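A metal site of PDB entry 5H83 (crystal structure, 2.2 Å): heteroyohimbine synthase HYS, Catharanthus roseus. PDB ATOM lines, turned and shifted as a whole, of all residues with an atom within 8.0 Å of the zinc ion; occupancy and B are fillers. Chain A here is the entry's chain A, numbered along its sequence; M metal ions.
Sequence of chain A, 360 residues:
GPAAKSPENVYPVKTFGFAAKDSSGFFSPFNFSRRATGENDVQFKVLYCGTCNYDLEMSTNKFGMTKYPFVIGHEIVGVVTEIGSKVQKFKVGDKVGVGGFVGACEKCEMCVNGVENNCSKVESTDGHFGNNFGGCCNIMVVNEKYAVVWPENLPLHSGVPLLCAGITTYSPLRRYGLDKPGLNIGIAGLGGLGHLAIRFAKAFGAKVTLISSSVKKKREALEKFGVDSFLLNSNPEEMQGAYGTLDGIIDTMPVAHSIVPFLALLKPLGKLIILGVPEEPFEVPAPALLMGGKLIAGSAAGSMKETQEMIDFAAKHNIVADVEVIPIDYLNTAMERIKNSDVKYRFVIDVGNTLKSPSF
SG of Cys 119 binds the zinc ion (2.3 Å). The zinc ion is bound by SG of Cys 111 (2.3 Å). SG of Cys 108 is bound to the zinc ion (2.3 Å). The side-chain sulfur (SG) of Cys 105 is bound to the zinc ion. The zinc ion has four donor atoms within binding distance.
N of Glu 106 touches the zinc ion (3.8 Å). Of the 19 residues printed, 5 come within 4 Å of the zinc ion. Along chain A the residues within 4 Å of the zinc ion span positions 105 to 119.
N of Met 110 sits close to SG of Cys 108, 3.5 Å away. SG of Cys 111 sits close to N of Glu 106, 3.2 Å away. N of Lys 107 lies close to SG of Cys 105 (3.5 Å). OE2 of Glu 106 sits at hydrogen-bond distance from OH of Tyr 146, at 2.7 Å. SG of Cys 119 sits close to N of Lys 121 (3.3 Å).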
ATOM      1  N   GLY A 103       9.690   1.552  -2.230  1.00  0.00           N
ATOM      2  CA  GLY A 103      11.100   1.219  -2.177  1.00  0.00           C
ATOM      3  C   GLY A 103      11.887   2.195  -1.339  1.00  0.00           C
ATOM      4  O   GLY A 103      11.382   3.248  -0.909  1.00  0.00           O
ATOM      5  N   ALA A 104      13.139   1.819  -1.095  1.00  0.00           N
ATOM      6  CA  ALA A 104      14.041   2.626  -0.287  1.00  0.00           C
ATOM      7  C   ALA A 104      15.422   2.030  -0.478  1.00  0.00           C
ATOM      8  O   ALA A 104      15.572   1.017  -1.167  1.00  0.00           O
ATOM      9  CB  ALA A 104      13.611   2.599   1.188  1.00  0.00           C
ATOM     10  N   CYS A 105      16.429   2.620   0.151  1.00  0.00           N
ATOM     11  CA  CYS A 105      17.823   2.248  -0.190  1.00  0.00           C
ATOM     12  C   CYS A 105      18.185   0.877   0.404  1.00  0.00           C
ATOM     13  O   CYS A 105      19.081   0.198  -0.114  1.00  0.00           O
ATOM     14  CB  CYS A 105      18.827   3.348   0.199  1.00  0.00           C
ATOM     15  SG  CYS A 105      19.398   3.282   1.900  1.00  0.00           S
ATOM     16  N   GLU A 106      17.464   0.478   1.448  1.00  0.00           N
ATOM     17  CA  GLU A 106      17.612  -0.843   2.104  1.00  0.00           C
ATOM     18  C   GLU A 106      18.912  -1.040   2.884  1.00  0.00           C
ATOM     19  O   GLU A 106      19.124  -2.117   3.415  1.00  0.00           O
ATOM     20  CB  GLU A 106      17.467  -2.009   1.111  1.00  0.00           C
ATOM     21  CG  GLU A 106      16.270  -1.958   0.161  1.00  0.00           C
ATOM     22  CD  GLU A 106      14.917  -2.113   0.860  1.00  0.00           C
ATOM     23  OE1 GLU A 106      14.878  -2.250   2.106  1.00  0.00           O
ATOM     24  OE2 GLU A 106      13.883  -2.118   0.138  1.00  0.00           O
ATOM     25  N   LYS A 107      19.746   0.005   2.986  1.00  0.00           N
ATOM     26  CA  LYS A 107      21.110  -0.102   3.536  1.00  0.00           C
ATOM     27  C   LYS A 107      21.447   0.942   4.655  1.00  0.00           C
ATOM     28  O   LYS A 107      22.375   0.720   5.437  1.00  0.00           O
ATOM     29  CB  LYS A 107      22.137   0.018   2.376  1.00  0.00           C
ATOM     30  CG  LYS A 107      22.443  -1.261   1.594  1.00  0.00           C
ATOM     31  N   CYS A 108      20.720   2.061   4.721  1.00  0.00           N
ATOM     32  CA  CYS A 108      20.976   3.107   5.701  1.00  0.00           C
ATOM     33  C   CYS A 108      20.417   2.750   7.103  1.00  0.00           C
ATOM     34  O   CYS A 108      19.691   1.774   7.279  1.00  0.00           O
ATOM     35  CB  CYS A 108      20.401   4.446   5.195  1.00  0.00           C
ATOM     36  SG  CYS A 108      18.598   4.624   5.375  1.00  0.00           S
ATOM     37  N   GLU A 109      20.801   3.544   8.089  1.00  0.00           N
ATOM     38  CA  GLU A 109      20.306   3.394   9.456  1.00  0.00           C
ATOM     39  C   GLU A 109      18.761   3.260   9.548  1.00  0.00           C
ATOM     40  O   GLU A 109      18.254   2.383  10.258  1.00  0.00           O
ATOM     41  CB  GLU A 109      20.780   4.576  10.262  1.00  0.00           C
ATOM     42  CG  GLU A 109      20.179   4.720  11.653  1.00  0.00           C
ATOM     43  CD  GLU A 109      20.636   6.014  12.287  1.00  0.00           C
ATOM     44  OE1 GLU A 109      21.763   6.055  12.817  1.00  0.00           O
ATOM     45  OE2 GLU A 109      19.882   7.006  12.210  1.00  0.00           O
ATOM     46  N   MET A 110      18.042   4.107   8.808  1.00  0.00           N
ATOM     47  CA  MET A 110      16.572   4.158   8.828  1.00  0.00           C
ATOM     48  C   MET A 110      15.980   2.865   8.298  1.00  0.00           C
ATOM     49  O   MET A 110      15.075   2.304   8.915  1.00  0.00           O
ATOM     50  CB  MET A 110      16.026   5.366   8.030  1.00  0.00           C
ATOM     51  CG  MET A 110      16.476   6.739   8.516  1.00  0.00           C
ATOM     52  SD  MET A 110      16.031   7.068  10.238  1.00  0.00           S
ATOM     53  CE  MET A 110      17.184   8.381  10.671  1.00  0.00           C
ATOM     54  N   CYS A 111      16.497   2.405   7.148  1.00  0.00           N
ATOM     55  CA  CYS A 111      16.054   1.151   6.510  1.00  0.00           C
ATOM     56  C   CYS A 111      16.372  -0.063   7.369  1.00  0.00           C
ATOM     57  O   CYS A 111      15.505  -0.870   7.638  1.00  0.00           O
ATOM     58  CB  CYS A 111      16.748   0.976   5.163  1.00  0.00           C
ATOM     59  SG  CYS A 111      16.098   2.088   3.911  1.00  0.00           S
ATOM     60  N   VAL A 112      17.622  -0.168   7.808  1.00  0.00           N
ATOM     61  CA  VAL A 112      18.080  -1.278   8.651  1.00  0.00           C
ATOM     62  C   VAL A 112      17.219  -1.436   9.903  1.00  0.00           C
ATOM     63  O   VAL A 112      16.936  -2.563  10.329  1.00  0.00           O
ATOM     64  CB  VAL A 112      19.596  -1.127   9.009  1.00  0.00           C
ATOM     65  CG1 VAL A 112      20.004  -1.880  10.270  1.00  0.00           C
ATOM     66  CG2 VAL A 112      20.451  -1.560   7.821  1.00  0.00           C
ATOM     67  N   VAL A 115      12.450   1.580   9.806  1.00  0.00           N
ATOM     68  CA  VAL A 115      11.779   2.883   9.650  1.00  0.00           C
ATOM     69  C   VAL A 115      12.144   3.516   8.299  1.00  0.00           C
ATOM     70  O   VAL A 115      12.393   4.732   8.179  1.00  0.00           O
ATOM     71  CB  VAL A 115      11.987   3.805  10.877  1.00  0.00           C
ATOM     72  CG1 VAL A 115      11.366   3.151  12.107  1.00  0.00           C
ATOM     73  CG2 VAL A 115      13.465   4.105  11.142  1.00  0.00           C
ATOM     74  N   GLU A 116      12.114   2.662   7.287  1.00  0.00           N
ATOM     75  CA  GLU A 116      12.496   3.013   5.907  1.00  0.00           C
ATOM     76  C   GLU A 116      11.657   4.118   5.254  1.00  0.00           C
ATOM     77  O   GLU A 116      12.093   4.713   4.255  1.00  0.00           O
ATOM     78  CB  GLU A 116      12.529   1.773   5.004  1.00  0.00           C
ATOM     79  CG  GLU A 116      11.183   1.181   4.606  1.00  0.00           C
ATOM     80  CD  GLU A 116      10.386   0.602   5.762  1.00  0.00           C
ATOM     81  OE1 GLU A 116      10.988   0.153   6.776  1.00  0.00           O
ATOM     82  OE2 GLU A 116       9.148   0.614   5.658  1.00  0.00           O
ATOM     83  N   ASN A 117      10.469   4.426   5.810  1.00  0.00           N
ATOM     84  CA  ASN A 117       9.728   5.648   5.417  1.00  0.00           C
ATOM     85  C   ASN A 117      10.549   6.932   5.572  1.00  0.00           C
ATOM     86  O   ASN A 117      10.298   7.905   4.845  1.00  0.00           O
ATOM     87  CB  ASN A 117       8.379   5.784   6.146  1.00  0.00           C
ATOM     88  CG  ASN A 117       8.499   5.711   7.662  1.00  0.00           C
ATOM     89  OD1 ASN A 117       9.220   4.876   8.208  1.00  0.00           O
ATOM     90  ND2 ASN A 117       7.772   6.572   8.364  1.00  0.00           N
ATOM     91  N   ASN A 118      11.524   6.933   6.502  1.00  0.00           N
ATOM     92  CA  ASN A 118      12.468   8.050   6.677  1.00  0.00           C
ATOM     93  C   ASN A 118      13.751   7.978   5.869  1.00  0.00           C
ATOM     94  O   ASN A 118      14.663   8.743   6.133  1.00  0.00           O
ATOM     95  CB  ASN A 118      12.836   8.177   8.164  1.00  0.00           C
ATOM     96  CG  ASN A 118      11.614   8.437   9.032  1.00  0.00           C
ATOM     97  OD1 ASN A 118      10.981   9.478   8.903  1.00  0.00           O
ATOM     98  ND2 ASN A 118      11.273   7.480   9.882  1.00  0.00           N
ATOM     99  N   CYS A 119      13.835   7.055   4.912  1.00  0.00           N
ATOM    100  CA  CYS A 119      15.045   6.926   4.089  1.00  0.00           C
ATOM    101  C   CYS A 119      15.130   8.170   3.240  1.00  0.00           C
ATOM    102  O   CYS A 119      14.139   8.586   2.642  1.00  0.00           O
ATOM    103  CB  CYS A 119      14.993   5.681   3.194  1.00  0.00           C
ATOM    104  SG  CYS A 119      16.502   5.369   2.217  1.00  0.00           S
ATOM    105  N   SER A 120      16.313   8.763   3.185  1.00  0.00           N
ATOM    106  CA  SER A 120      16.547   9.877   2.276  1.00  0.00           C
ATOM    107  C   SER A 120      16.349   9.458   0.795  1.00  0.00           C
ATOM    108  O   SER A 120      16.103  10.320  -0.051  1.00  0.00           O
ATOM    109  CB  SER A 120      17.938  10.457   2.503  1.00  0.00           C
ATOM    110  OG  SER A 120      18.889   9.466   2.198  1.00  0.00           O
ATOM    111  N   LYS A 121      16.447   8.169   0.492  1.00  0.00           N
ATOM    112  CA  LYS A 121      16.210   7.654  -0.879  1.00  0.00           C
ATOM    113  C   LYS A 121      14.899   6.856  -1.000  1.00  0.00           C
ATOM    114  O   LYS A 121      14.755   6.018  -1.895  1.00  0.00           O
ATOM    115  CB  LYS A 121      17.443   6.858  -1.354  1.00  0.00           C
ATOM    116  CG  LYS A 121      18.671   7.734  -1.614  1.00  0.00           C
ATOM    117  CD  LYS A 121      19.849   6.949  -2.192  1.00  0.00           C
ATOM    118  N   VAL A 122      13.919   7.175  -0.145  1.00  0.00           N
ATOM    119  CA  VAL A 122      12.597   6.525  -0.200  1.00  0.00           C
ATOM    120  C   VAL A 122      11.965   6.775  -1.576  1.00  0.00           C
ATOM    121  O   VAL A 122      12.135   7.853  -2.163  1.00  0.00           O
ATOM    122  CB  VAL A 122      11.680   7.018   0.973  1.00  0.00           C
ATOM    123  CG1 VAL A 122      11.236   8.467   0.793  1.00  0.00           C
ATOM    124  CG2 VAL A 122      10.457   6.101   1.139  1.00  0.00           C
ATOM    125  N   TYR A 146       7.039  -4.144   0.144  1.00  0.00           N
ATOM    126  CA  TYR A 146       6.258  -2.927   0.244  1.00  0.00           C
ATOM    127  C   TYR A 146       4.797  -3.162   0.009  1.00  0.00           C
ATOM    128  O   TYR A 146       4.069  -2.203  -0.159  1.00  0.00           O
ATOM    129  CB  TYR A 146       6.859  -1.871  -0.693  1.00  0.00           C
ATOM    130  CG  TYR A 146       8.243  -1.567  -0.197  1.00  0.00           C
ATOM    131  CD1 TYR A 146       8.412  -0.755   0.911  1.00  0.00           C
ATOM    132  CD2 TYR A 146       9.350  -2.196  -0.711  1.00  0.00           C
ATOM    133  CE1 TYR A 146       9.647  -0.511   1.451  1.00  0.00           C
ATOM    134  CE2 TYR A 146      10.610  -1.948  -0.192  1.00  0.00           C
ATOM    135  CZ  TYR A 146      10.741  -1.093   0.903  1.00  0.00           C
ATOM    136  OH  TYR A 146      11.951  -0.790   1.480  1.00  0.00           O
HETATM  137 ZN    ZN M   1      17.647   3.768   3.413  1.00  0.00          ZN
